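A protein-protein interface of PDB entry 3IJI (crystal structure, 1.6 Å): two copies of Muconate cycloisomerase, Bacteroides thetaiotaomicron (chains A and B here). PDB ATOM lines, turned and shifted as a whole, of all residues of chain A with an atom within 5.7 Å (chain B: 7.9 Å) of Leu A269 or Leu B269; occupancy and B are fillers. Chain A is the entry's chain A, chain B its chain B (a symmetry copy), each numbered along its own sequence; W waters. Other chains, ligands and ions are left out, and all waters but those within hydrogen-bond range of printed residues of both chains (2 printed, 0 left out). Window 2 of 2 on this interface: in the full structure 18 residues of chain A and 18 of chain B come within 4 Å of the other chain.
The backbone carbonyl oxygen (O) of Trp A264 sits at hydrogen-bond distance from the side-chain hydroxyl (OG1) of Thr A268, at 3.2 Å. The backbone carbonyl oxygen (O) of Trp B264 is in hydrogen-bond range of the side-chain hydroxyl (OG1) of Thr B268.
Among the printed residues, merely in contact across the chains: Lys A265 with Thr B268 (3.8 Å), Thr A268 with Lys B265 (3.9 Å), Leu A269 with Leu B269 (3.4 Å), Leu A269 with Ala B272 (3.9 Å) and Ala A272 with Leu B269 (3.8 Å).
Printed residues of chain B within 4 Å of Lys A265: Thr B268 (3.8 Å). Of the printed residues of chain B, Thr A268 touches Lys B265 (3.9 Å). Leu A269 touches two residues of chain B. Printed residues of chain B within 4 Å of Ala A272: Leu B269. Leu A273 touches none of the printed residues of chain B. Printed residues of chain A within 4 Å of Lys B265: Thr A268. Of the printed residues of chain A, Thr B268 touches Lys A265 (3.8 Å). Leu B269 touches just these residues of chain A: Leu A269 and Ala A272. The nearest residue of chain B that does not touch Leu A269 is Leu B273 (4.4 Å). The nearest residue of chain A that does not touch Leu B269 is Leu A273 (4.6 Å).
Printed residues of chain B that touch a printed residue of chain A: Lys B265, Thr B268, Leu B269 and Ala B272. Of the 14 printed residues of chain A, 4 touch a printed residue of chain B. Among the printed residues, no Asp or Glu carboxylate lies within 4 Å of a Lys or Arg side-chain nitrogen of the other chain.
Lys A265 touches Thr B268, and with the chains exchanged Thr A268 touches Lys B265. Leu B269 touches its own counterpart, Leu A269. Leu A269 touches Ala B272, and with the chains exchanged Ala A272 touches Leu B269. 14 positions are printed for both chains. Of the 5 pairs that touch across the chains among the printed residues, 5 have their exchanged pair printed and touching as well.
Water W1 bridges OG1 of Thr B268 (2.8 Å) and OG1 of Thr A268 (2.9 Å). Water W2 bridges NE1 of Trp A264 and NE1 of Trp B264.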
ATOM      1  N   LEU A 237     -37.634 -20.140   3.270  1.00  0.00           N
ATOM      2  CA  LEU A 237     -36.920 -20.859   2.221  1.00  0.00           C
ATOM      3  C   LEU A 237     -37.848 -21.383   1.125  1.00  0.00           C
ATOM      4  O   LEU A 237     -37.549 -21.266  -0.062  1.00  0.00           O
ATOM      5  CB  LEU A 237     -36.152 -22.030   2.841  1.00  0.00           C
ATOM      6  CG  LEU A 237     -35.225 -22.848   1.938  1.00  0.00           C
ATOM      7  CD1 LEU A 237     -34.112 -21.967   1.400  1.00  0.00           C
ATOM      8  CD2 LEU A 237     -34.647 -24.003   2.740  1.00  0.00           C
ATOM      9  N   VAL A 240     -38.812 -18.853  -1.839  1.00  0.00           N
ATOM     10  CA  VAL A 240     -37.812 -18.272  -2.729  1.00  0.00           C
ATOM     11  C   VAL A 240     -37.879 -18.642  -4.213  1.00  0.00           C
ATOM     12  O   VAL A 240     -37.951 -17.763  -5.073  1.00  0.00           O
ATOM     13  CB  VAL A 240     -36.390 -18.592  -2.221  1.00  0.00           C
ATOM     14  CG1 VAL A 240     -35.353 -18.005  -3.168  1.00  0.00           C
ATOM     15  CG2 VAL A 240     -36.200 -18.032  -0.818  1.00  0.00           C
ATOM     16  N   ALA A 241     -37.839 -19.937  -4.510  1.00  0.00           N
ATOM     17  CA  ALA A 241     -37.855 -20.411  -5.892  1.00  0.00           C
ATOM     18  C   ALA A 241     -38.927 -19.785  -6.784  1.00  0.00           C
ATOM     19  O   ALA A 241     -38.662 -19.455  -7.941  1.00  0.00           O
ATOM     20  CB  ALA A 241     -37.988 -21.929  -5.915  1.00  0.00           C
ATOM     21  N   TRP A 264     -29.234 -18.879   6.052  1.00  0.00           N
ATOM     22  CA  TRP A 264     -28.066 -19.259   5.259  1.00  0.00           C
ATOM     23  C   TRP A 264     -28.473 -20.141   4.081  1.00  0.00           C
ATOM     24  O   TRP A 264     -27.879 -20.058   3.009  1.00  0.00           O
ATOM     25  CB  TRP A 264     -27.033 -19.978   6.135  1.00  0.00           C
ATOM     26  CG  TRP A 264     -25.690 -20.165   5.463  1.00  0.00           C
ATOM     27  CD1 TRP A 264     -24.957 -21.313   5.416  1.00  0.00           C
ATOM     28  CD2 TRP A 264     -24.920 -19.169   4.767  1.00  0.00           C
ATOM     29  NE1 TRP A 264     -23.778 -21.099   4.738  1.00  0.00           N
ATOM     30  CE2 TRP A 264     -23.730 -19.793   4.328  1.00  0.00           C
ATOM     31  CE3 TRP A 264     -25.120 -17.812   4.472  1.00  0.00           C
ATOM     32  CZ2 TRP A 264     -22.739 -19.107   3.608  1.00  0.00           C
ATOM     33  CZ3 TRP A 264     -24.134 -17.127   3.754  1.00  0.00           C
ATOM     34  CH2 TRP A 264     -22.958 -17.781   3.332  1.00  0.00           C
ATOM     35  N   LYS A 265     -29.480 -20.987   4.277  1.00  0.00           N
ATOM     36  CA  LYS A 265     -29.952 -21.835   3.187  1.00  0.00           C
ATOM     37  C   LYS A 265     -30.605 -20.957   2.123  1.00  0.00           C
ATOM     38  O   LYS A 265     -30.517 -21.246   0.929  1.00  0.00           O
ATOM     39  CB  LYS A 265     -30.970 -22.859   3.691  1.00  0.00           C
ATOM     40  CG  LYS A 265     -30.416 -23.867   4.672  1.00  0.00           C
ATOM     41  CD  LYS A 265     -31.478 -24.910   4.970  1.00  0.00           C
ATOM     42  CE  LYS A 265     -31.128 -25.738   6.177  1.00  0.00           C
ATOM     43  NZ  LYS A 265     -32.159 -26.788   6.384  1.00  0.00           N
ATOM     44  N   MET A 266     -31.263 -19.884   2.555  1.00  0.00           N
ATOM     45  CA  MET A 266     -31.918 -18.979   1.616  1.00  0.00           C
ATOM     46  C   MET A 266     -30.883 -18.257   0.761  1.00  0.00           C
ATOM     47  O   MET A 266     -31.113 -18.007  -0.420  1.00  0.00           O
ATOM     48  CB  MET A 266     -32.794 -17.973   2.368  1.00  0.00           C
ATOM     49  CG  MET A 266     -34.006 -18.623   3.018  1.00  0.00           C
ATOM     50  SD  MET A 266     -34.964 -17.510   4.064  1.00  0.00           S
ATOM     51  CE  MET A 266     -35.900 -16.581   2.848  1.00  0.00           C
ATOM     52  N   VAL A 267     -29.743 -17.919   1.359  1.00  0.00           N
ATOM     53  CA  VAL A 267     -28.678 -17.252   0.618  1.00  0.00           C
ATOM     54  C   VAL A 267     -28.182 -18.212  -0.459  1.00  0.00           C
ATOM     55  O   VAL A 267     -28.017 -17.835  -1.619  1.00  0.00           O
ATOM     56  CB  VAL A 267     -27.494 -16.878   1.538  1.00  0.00           C
ATOM     57  CG1 VAL A 267     -26.331 -16.346   0.703  1.00  0.00           C
ATOM     58  CG2 VAL A 267     -27.937 -15.837   2.555  1.00  0.00           C
ATOM     59  N   THR A 268     -27.951 -19.461  -0.068  1.00  0.00           N
ATOM     60  CA  THR A 268     -27.477 -20.477  -0.999  1.00  0.00           C
ATOM     61  C   THR A 268     -28.452 -20.673  -2.152  1.00  0.00           C
ATOM     62  O   THR A 268     -28.056 -20.701  -3.317  1.00  0.00           O
ATOM     63  CB  THR A 268     -27.279 -21.833  -0.290  1.00  0.00           C
ATOM     64  OG1 THR A 268     -26.315 -21.685   0.756  1.00  0.00           O
ATOM     65  CG2 THR A 268     -26.794 -22.886  -1.272  1.00  0.00           C
ATOM     66  N   LEU A 269     -29.732 -20.810  -1.822  1.00  0.00           N
ATOM     67  CA  LEU A 269     -30.766 -21.013  -2.826  1.00  0.00           C
ATOM     68  C   LEU A 269     -30.881 -19.837  -3.793  1.00  0.00           C
ATOM     69  O   LEU A 269     -30.923 -20.027  -5.006  1.00  0.00           O
ATOM     70  CB  LEU A 269     -32.114 -21.261  -2.146  1.00  0.00           C
ATOM     71  CG  LEU A 269     -33.324 -21.476  -3.057  1.00  0.00           C
ATOM     72  CD1 LEU A 269     -33.068 -22.651  -3.994  1.00  0.00           C
ATOM     73  CD2 LEU A 269     -34.557 -21.730  -2.208  1.00  0.00           C
ATOM     74  N   ALA A 270     -30.934 -18.620  -3.259  1.00  0.00           N
ATOM     75  CA  ALA A 270     -31.044 -17.438  -4.103  1.00  0.00           C
ATOM     76  C   ALA A 270     -29.861 -17.354  -5.066  1.00  0.00           C
ATOM     77  O   ALA A 270     -30.045 -17.216  -6.278  1.00  0.00           O
ATOM     78  CB  ALA A 270     -31.112 -16.180  -3.237  1.00  0.00           C
ATOM     79  N   HIS A 271     -28.651 -17.441  -4.523  1.00  0.00           N
ATOM     80  CA  HIS A 271     -27.437 -17.372  -5.333  1.00  0.00           C
ATOM     81  C   HIS A 271     -27.378 -18.484  -6.369  1.00  0.00           C
ATOM     82  O   HIS A 271     -27.046 -18.243  -7.532  1.00  0.00           O
ATOM     83  CB  HIS A 271     -26.199 -17.434  -4.436  1.00  0.00           C
ATOM     84  CG  HIS A 271     -25.888 -16.144  -3.745  1.00  0.00           C
ATOM     85  ND1 HIS A 271     -24.897 -16.028  -2.794  1.00  0.00           N
ATOM     86  CD2 HIS A 271     -26.419 -14.907  -3.887  1.00  0.00           C
ATOM     87  CE1 HIS A 271     -24.831 -14.775  -2.382  1.00  0.00           C
ATOM     88  NE2 HIS A 271     -25.743 -14.073  -3.031  1.00  0.00           N
ATOM     89  N   ALA A 272     -27.703 -19.700  -5.947  1.00  0.00           N
ATOM     90  CA  ALA A 272     -27.684 -20.839  -6.854  1.00  0.00           C
ATOM     91  C   ALA A 272     -28.657 -20.604  -8.002  1.00  0.00           C
ATOM     92  O   ALA A 272     -28.447 -21.088  -9.114  1.00  0.00           O
ATOM     93  CB  ALA A 272     -28.052 -22.115  -6.106  1.00  0.00           C
ATOM     94  N   LEU A 273     -29.721 -19.851  -7.729  1.00  0.00           N
ATOM     95  CA  LEU A 273     -30.731 -19.548  -8.738  1.00  0.00           C
ATOM     96  C   LEU A 273     -30.465 -18.248  -9.496  1.00  0.00           C
ATOM     97  O   LEU A 273     -31.327 -17.771 -10.236  1.00  0.00           O
ATOM     98  CB  LEU A 273     -32.119 -19.470  -8.098  1.00  0.00           C
ATOM     99  CG  LEU A 273     -32.730 -20.766  -7.559  1.00  0.00           C
ATOM    100  CD1 LEU A 273     -34.098 -20.468  -6.963  1.00  0.00           C
ATOM    101  CD2 LEU A 273     -32.851 -21.788  -8.681  1.00  0.00           C
ATOM    102  N   GLY A 274     -29.286 -17.669  -9.297  1.00  0.00           N
ATOM    103  CA  GLY A 274     -28.942 -16.437  -9.988  1.00  0.00           C
ATOM    104  C   GLY A 274     -29.599 -15.181  -9.447  1.00  0.00           C
ATOM    105  O   GLY A 274     -29.666 -14.164 -10.139  1.00  0.00           O
ATOM    106  N   ARG B 236     -22.166 -30.033 -11.499  1.00  0.00           N
ATOM    107  CA  ARG B 236     -22.033 -29.009 -10.471  1.00  0.00           C
ATOM    108  C   ARG B 236     -23.322 -28.334 -10.033  1.00  0.00           C
ATOM    109  O   ARG B 236     -24.405 -28.627 -10.542  1.00  0.00           O
ATOM    110  CB  ARG B 236     -21.047 -27.945 -10.951  1.00  0.00           C
ATOM    111  CG  ARG B 236     -19.694 -28.518 -11.316  1.00  0.00           C
ATOM    112  CD  ARG B 236     -18.689 -27.429 -11.612  1.00  0.00           C
ATOM    113  NE  ARG B 236     -18.539 -26.526 -10.478  1.00  0.00           N
ATOM    114  CZ  ARG B 236     -17.615 -25.578 -10.394  1.00  0.00           C
ATOM    115  NH1 ARG B 236     -16.749 -25.403 -11.388  1.00  0.00           N
ATOM    116  NH2 ARG B 236     -17.556 -24.804  -9.319  1.00  0.00           N
ATOM    117  N   LEU B 237     -23.175 -27.415  -9.085  1.00  0.00           N
ATOM    118  CA  LEU B 237     -24.292 -26.666  -8.521  1.00  0.00           C
ATOM    119  C   LEU B 237     -25.180 -26.027  -9.588  1.00  0.00           C
ATOM    120  O   LEU B 237     -26.406 -26.086  -9.499  1.00  0.00           O
ATOM    121  CB  LEU B 237     -23.754 -25.586  -7.583  1.00  0.00           C
ATOM    122  CG  LEU B 237     -24.769 -24.760  -6.796  1.00  0.00           C
ATOM    123  CD1 LEU B 237     -25.623 -25.675  -5.924  1.00  0.00           C
ATOM    124  CD2 LEU B 237     -24.027 -23.739  -5.947  1.00  0.00           C
ATOM    125  N   GLY B 238     -24.556 -25.428 -10.599  1.00  0.00           N
ATOM    126  CA  GLY B 238     -25.311 -24.772 -11.653  1.00  0.00           C
ATOM    127  C   GLY B 238     -26.095 -25.680 -12.582  1.00  0.00           C
ATOM    128  O   GLY B 238     -26.829 -25.198 -13.443  1.00  0.00           O
ATOM    129  N   ASP B 239     -25.948 -26.993 -12.417  1.00  0.00           N
ATOM    130  CA  ASP B 239     -26.656 -27.949 -13.265  1.00  0.00           C
ATOM    131  C   ASP B 239     -27.886 -28.554 -12.589  1.00  0.00           C
ATOM    132  O   ASP B 239     -28.663 -29.263 -13.228  1.00  0.00           O
ATOM    133  CB  ASP B 239     -25.730 -29.105 -13.667  1.00  0.00           C
ATOM    134  CG  ASP B 239     -24.433 -28.636 -14.289  1.00  0.00           C
ATOM    135  OD1 ASP B 239     -24.451 -27.629 -15.022  1.00  0.00           O
ATOM    136  OD2 ASP B 239     -23.397 -29.293 -14.057  1.00  0.00           O
ATOM    137  N   VAL B 240     -28.068 -28.266 -11.305  1.00  0.00           N
ATOM    138  CA  VAL B 240     -29.172 -28.847 -10.542  1.00  0.00           C
ATOM    139  C   VAL B 240     -30.594 -28.388 -10.866  1.00  0.00           C
ATOM    140  O   VAL B 240     -31.468 -29.217 -11.128  1.00  0.00           O
ATOM    141  CB  VAL B 240     -28.943 -28.650  -9.026  1.00  0.00           C
ATOM    142  CG1 VAL B 240     -30.100 -29.265  -8.238  1.00  0.00           C
ATOM    143  CG2 VAL B 240     -27.622 -29.288  -8.612  1.00  0.00           C
ATOM    144  N   ALA B 241     -30.824 -27.081 -10.839  1.00  0.00           N
ATOM    145  CA  ALA B 241     -32.155 -26.531 -11.088  1.00  0.00           C
ATOM    146  C   ALA B 241     -32.853 -27.025 -12.352  1.00  0.00           C
ATOM    147  O   ALA B 241     -34.060 -27.268 -12.342  1.00  0.00           O
ATOM    148  CB  ALA B 241     -32.087 -25.012 -11.101  1.00  0.00           C
ATOM    149  N   ALA B 242     -32.102 -27.174 -13.436  1.00  0.00           N
ATOM    150  CA  ALA B 242     -32.675 -27.617 -14.703  1.00  0.00           C
ATOM    151  C   ALA B 242     -33.229 -29.038 -14.674  1.00  0.00           C
ATOM    152  O   ALA B 242     -33.962 -29.440 -15.576  1.00  0.00           O
ATOM    153  CB  ALA B 242     -31.636 -27.497 -15.806  1.00  0.00           C
ATOM    154  N   LYS B 244     -35.071 -30.293 -12.079  1.00  0.00           N
ATOM    155  CA  LYS B 244     -36.300 -30.363 -11.303  1.00  0.00           C
ATOM    156  C   LYS B 244     -37.447 -30.739 -12.234  1.00  0.00           C
ATOM    157  O   LYS B 244     -37.604 -30.152 -13.306  1.00  0.00           O
ATOM    158  CB  LYS B 244     -36.598 -29.017 -10.642  1.00  0.00           C
ATOM    159  CG  LYS B 244     -37.942 -28.981  -9.934  1.00  0.00           C
ATOM    160  CD  LYS B 244     -38.223 -27.626  -9.318  1.00  0.00           C
ATOM    161  CE  LYS B 244     -39.618 -27.592  -8.715  1.00  0.00           C
ATOM    162  NZ  LYS B 244     -39.825 -28.699  -7.737  1.00  0.00           N
ATOM    163  N   ILE B 250     -30.852 -36.081  -7.142  1.00  0.00           N
ATOM    164  CA  ILE B 250     -29.542 -35.939  -7.770  1.00  0.00           C
ATOM    165  C   ILE B 250     -28.468 -36.737  -7.048  1.00  0.00           C
ATOM    166  O   ILE B 250     -28.575 -36.993  -5.851  1.00  0.00           O
ATOM    167  CB  ILE B 250     -29.082 -34.458  -7.803  1.00  0.00           C
ATOM    168  CG1 ILE B 250     -28.909 -33.920  -6.375  1.00  0.00           C
ATOM    169  CG2 ILE B 250     -30.100 -33.612  -8.562  1.00  0.00           C
ATOM    170  CD1 ILE B 250     -28.245 -32.544  -6.313  1.00  0.00           C
ATOM    171  N   ILE B 252     -24.503 -36.720  -6.069  1.00  0.00           N
ATOM    172  CA  ILE B 252     -23.379 -35.804  -5.912  1.00  0.00           C
ATOM    173  C   ILE B 252     -22.082 -36.583  -5.739  1.00  0.00           C
ATOM    174  O   ILE B 252     -22.037 -37.555  -4.986  1.00  0.00           O
ATOM    175  CB  ILE B 252     -23.560 -34.924  -4.651  1.00  0.00           C
ATOM    176  CG1 ILE B 252     -24.814 -34.063  -4.784  1.00  0.00           C
ATOM    177  CG2 ILE B 252     -22.320 -34.058  -4.427  1.00  0.00           C
ATOM    178  CD1 ILE B 252     -25.218 -33.380  -3.482  1.00  0.00           C
ATOM    179  N   GLU B 262     -19.074 -27.096  -2.391  1.00  0.00           N
ATOM    180  CA  GLU B 262     -20.101 -27.073  -3.416  1.00  0.00           C
ATOM    181  C   GLU B 262     -21.076 -28.231  -3.211  1.00  0.00           C
ATOM    182  O   GLU B 262     -22.271 -28.093  -3.467  1.00  0.00           O
ATOM    183  CB  GLU B 262     -19.469 -27.138  -4.810  1.00  0.00           C
ATOM    184  CG  GLU B 262     -20.490 -27.138  -5.938  1.00  0.00           C
ATOM    185  CD  GLU B 262     -20.020 -26.381  -7.167  1.00  0.00           C
ATOM    186  OE1 GLU B 262     -20.568 -26.631  -8.257  1.00  0.00           O
ATOM    187  OE2 GLU B 262     -19.117 -25.524  -7.044  1.00  0.00           O
ATOM    188  N   ALA B 263     -20.571 -29.371  -2.744  1.00  0.00           N
ATOM    189  CA  ALA B 263     -21.424 -30.528  -2.508  1.00  0.00           C
ATOM    190  C   ALA B 263     -22.521 -30.178  -1.518  1.00  0.00           C
ATOM    191  O   ALA B 263     -23.693 -30.486  -1.738  1.00  0.00           O
ATOM    192  CB  ALA B 263     -20.602 -31.696  -1.970  1.00  0.00           C
ATOM    193  N   TRP B 264     -22.139 -29.524  -0.427  1.00  0.00           N
ATOM    194  CA  TRP B 264     -23.115 -29.162   0.590  1.00  0.00           C
ATOM    195  C   TRP B 264     -24.122 -28.153   0.043  1.00  0.00           C
ATOM    196  O   TRP B 264     -25.294 -28.172   0.420  1.00  0.00           O
ATOM    197  CB  TRP B 264     -22.412 -28.612   1.833  1.00  0.00           C
ATOM    198  CG  TRP B 264     -23.322 -28.507   3.032  1.00  0.00           C
ATOM    199  CD1 TRP B 264     -23.466 -27.431   3.856  1.00  0.00           C
ATOM    200  CD2 TRP B 264     -24.210 -29.519   3.536  1.00  0.00           C
ATOM    201  NE1 TRP B 264     -24.389 -27.705   4.840  1.00  0.00           N
ATOM    202  CE2 TRP B 264     -24.860 -28.978   4.668  1.00  0.00           C
ATOM    203  CE3 TRP B 264     -24.520 -30.828   3.140  1.00  0.00           C
ATOM    204  CZ2 TRP B 264     -25.803 -29.702   5.411  1.00  0.00           C
ATOM    205  CZ3 TRP B 264     -25.461 -31.549   3.879  1.00  0.00           C
ATOM    206  CH2 TRP B 264     -26.089 -30.979   5.002  1.00  0.00           C
ATOM    207  N   LYS B 265     -23.671 -27.267  -0.842  1.00  0.00           N
ATOM    208  CA  LYS B 265     -24.585 -26.300  -1.439  1.00  0.00           C
ATOM    209  C   LYS B 265     -25.566 -27.045  -2.345  1.00  0.00           C
ATOM    210  O   LYS B 265     -26.730 -26.660  -2.467  1.00  0.00           O
ATOM    211  CB  LYS B 265     -23.825 -25.262  -2.275  1.00  0.00           C
ATOM    212  CG  LYS B 265     -22.938 -24.331  -1.477  1.00  0.00           C
ATOM    213  CD  LYS B 265     -22.326 -23.294  -2.405  1.00  0.00           C
ATOM    214  CE  LYS B 265     -21.197 -22.543  -1.751  1.00  0.00           C
ATOM    215  NZ  LYS B 265     -20.672 -21.497  -2.675  1.00  0.00           N
ATOM    216  N   MET B 266     -25.092 -28.108  -2.992  1.00  0.00           N
ATOM    217  CA  MET B 266     -25.955 -28.889  -3.875  1.00  0.00           C
ATOM    218  C   MET B 266     -27.027 -29.627  -3.080  1.00  0.00           C
ATOM    219  O   MET B 266     -28.157 -29.782  -3.546  1.00  0.00           O
ATOM    220  CB  MET B 266     -25.125 -29.874  -4.703  1.00  0.00           C
ATOM    221  CG  MET B 266     -24.292 -29.189  -5.770  1.00  0.00           C
ATOM    222  SD  MET B 266     -23.097 -30.288  -6.561  1.00  0.00           S
ATOM    223  CE  MET B 266     -24.129 -31.140  -7.741  1.00  0.00           C
ATOM    224  N   VAL B 267     -26.669 -30.088  -1.885  1.00  0.00           N
ATOM    225  CA  VAL B 267     -27.623 -30.779  -1.025  1.00  0.00           C
ATOM    226  C   VAL B 267     -28.703 -29.777  -0.634  1.00  0.00           C
ATOM    227  O   VAL B 267     -29.895 -30.066  -0.707  1.00  0.00           O
ATOM    228  CB  VAL B 267     -26.955 -31.299   0.265  1.00  0.00           C
ATOM    229  CG1 VAL B 267     -28.016 -31.834   1.226  1.00  0.00           C
ATOM    230  CG2 VAL B 267     -25.955 -32.384  -0.070  1.00  0.00           C
ATOM    231  N   THR B 268     -28.269 -28.591  -0.222  1.00  0.00           N
ATOM    232  CA  THR B 268     -29.194 -27.545   0.183  1.00  0.00           C
ATOM    233  C   THR B 268     -30.122 -27.160  -0.965  1.00  0.00           C
ATOM    234  O   THR B 268     -31.335 -27.044  -0.781  1.00  0.00           O
ATOM    235  CB  THR B 268     -28.424 -26.294   0.671  1.00  0.00           C
ATOM    236  OG1 THR B 268     -27.550 -26.667   1.741  1.00  0.00           O
ATOM    237  CG2 THR B 268     -29.384 -25.232   1.161  1.00  0.00           C
ATOM    238  N   LEU B 269     -29.558 -26.985  -2.157  1.00  0.00           N
ATOM    239  CA  LEU B 269     -30.346 -26.604  -3.321  1.00  0.00           C
ATOM    240  C   LEU B 269     -31.352 -27.680  -3.722  1.00  0.00           C
ATOM    241  O   LEU B 269     -32.529 -27.391  -3.929  1.00  0.00           O
ATOM    242  CB  LEU B 269     -29.429 -26.293  -4.506  1.00  0.00           C
ATOM    243  CG  LEU B 269     -30.133 -25.978  -5.828  1.00  0.00           C
ATOM    244  CD1 LEU B 269     -31.056 -24.774  -5.658  1.00  0.00           C
ATOM    245  CD2 LEU B 269     -29.096 -25.710  -6.904  1.00  0.00           C
ATOM    246  N   ALA B 270     -30.889 -28.919  -3.833  1.00  0.00           N
ATOM    247  CA  ALA B 270     -31.771 -30.013  -4.212  1.00  0.00           C
ATOM    248  C   ALA B 270     -32.952 -30.115  -3.249  1.00  0.00           C
ATOM    249  O   ALA B 270     -34.102 -30.171  -3.679  1.00  0.00           O
ATOM    250  CB  ALA B 270     -30.995 -31.326  -4.233  1.00  0.00           C
ATOM    251  N   HIS B 271     -32.659 -30.139  -1.952  1.00  0.00           N
ATOM    252  CA  HIS B 271     -33.700 -30.241  -0.932  1.00  0.00           C
ATOM    253  C   HIS B 271     -34.665 -29.070  -0.974  1.00  0.00           C
ATOM    254  O   HIS B 271     -35.882 -29.258  -0.915  1.00  0.00           O
ATOM    255  CB  HIS B 271     -33.071 -30.348   0.457  1.00  0.00           C
ATOM    256  CG  HIS B 271     -32.549 -31.715   0.772  1.00  0.00           C
ATOM    257  ND1 HIS B 271     -31.797 -31.986   1.895  1.00  0.00           N
ATOM    258  CD2 HIS B 271     -32.691 -32.893   0.121  1.00  0.00           C
ATOM    259  CE1 HIS B 271     -31.498 -33.272   1.921  1.00  0.00           C
ATOM    260  NE2 HIS B 271     -32.029 -33.846   0.856  1.00  0.00           N
ATOM    261  N   ALA B 272     -34.118 -27.865  -1.075  1.00  0.00           N
ATOM    262  CA  ALA B 272     -34.938 -26.666  -1.135  1.00  0.00           C
ATOM    263  C   ALA B 272     -35.879 -26.743  -2.331  1.00  0.00           C
ATOM    264  O   ALA B 272     -36.960 -26.153  -2.316  1.00  0.00           O
ATOM    265  CB  ALA B 272     -34.053 -25.430  -1.241  1.00  0.00           C
ATOM    266  N   LEU B 273     -35.466 -27.475  -3.363  1.00  0.00           N
ATOM    267  CA  LEU B 273     -36.271 -27.631  -4.574  1.00  0.00           C
ATOM    268  C   LEU B 273     -37.147 -28.886  -4.568  1.00  0.00           C
ATOM    269  O   LEU B 273     -37.743 -29.236  -5.587  1.00  0.00           O
ATOM    270  CB  LEU B 273     -35.371 -27.664  -5.813  1.00  0.00           C
ATOM    271  CG  LEU B 273     -34.613 -26.388  -6.193  1.00  0.00           C
ATOM    272  CD1 LEU B 273     -33.749 -26.663  -7.417  1.00  0.00           C
ATOM    273  CD2 LEU B 273     -35.599 -25.262  -6.480  1.00  0.00           C
ATOM    274  N   GLY B 274     -37.211 -29.568  -3.429  1.00  0.00           N
ATOM    275  CA  GLY B 274     -38.031 -30.766  -3.327  1.00  0.00           C
ATOM    276  C   GLY B 274     -37.471 -32.021  -3.978  1.00  0.00           C
ATOM    277  O   GLY B 274     -38.209 -32.973  -4.233  1.00  0.00           O
ATOM    278  N   MET B 275     -36.170 -32.028  -4.252  1.00  0.00           N
ATOM    279  CA  MET B 275     -35.525 -33.185  -4.867  1.00  0.00           C
ATOM    280  C   MET B 275     -34.774 -33.977  -3.806  1.00  0.00           C
ATOM    281  O   MET B 275     -34.357 -33.420  -2.792  1.00  0.00           O
ATOM    282  CB  MET B 275     -34.530 -32.738  -5.939  1.00  0.00           C
ATOM    283  CG  MET B 275     -35.152 -32.048  -7.133  1.00  0.00           C
ATOM    284  SD  MET B 275     -33.895 -31.541  -8.322  1.00  0.00           S
ATOM    285  CE  MET B 275     -33.796 -32.974  -9.332  1.00  0.00           C
ATOM    286  N   VAL B 277     -31.560 -36.574  -2.554  1.00  0.00           N
ATOM    287  CA  VAL B 277     -30.121 -36.558  -2.777  1.00  0.00           C
ATOM    288  C   VAL B 277     -29.463 -37.890  -2.461  1.00  0.00           C
ATOM    289  O   VAL B 277     -29.862 -38.592  -1.535  1.00  0.00           O
ATOM    290  CB  VAL B 277     -29.438 -35.478  -1.891  1.00  0.00           C
ATOM    291  CG1 VAL B 277     -27.920 -35.516  -2.082  1.00  0.00           C
ATOM    292  CG2 VAL B 277     -29.986 -34.100  -2.227  1.00  0.00           C
HETATM  293  O   HOH W   1     -25.925 -24.359   1.730  1.00  0.00           O
HETATM  294  O   HOH W   2     -23.678 -24.328   5.206  1.00  0.00           O
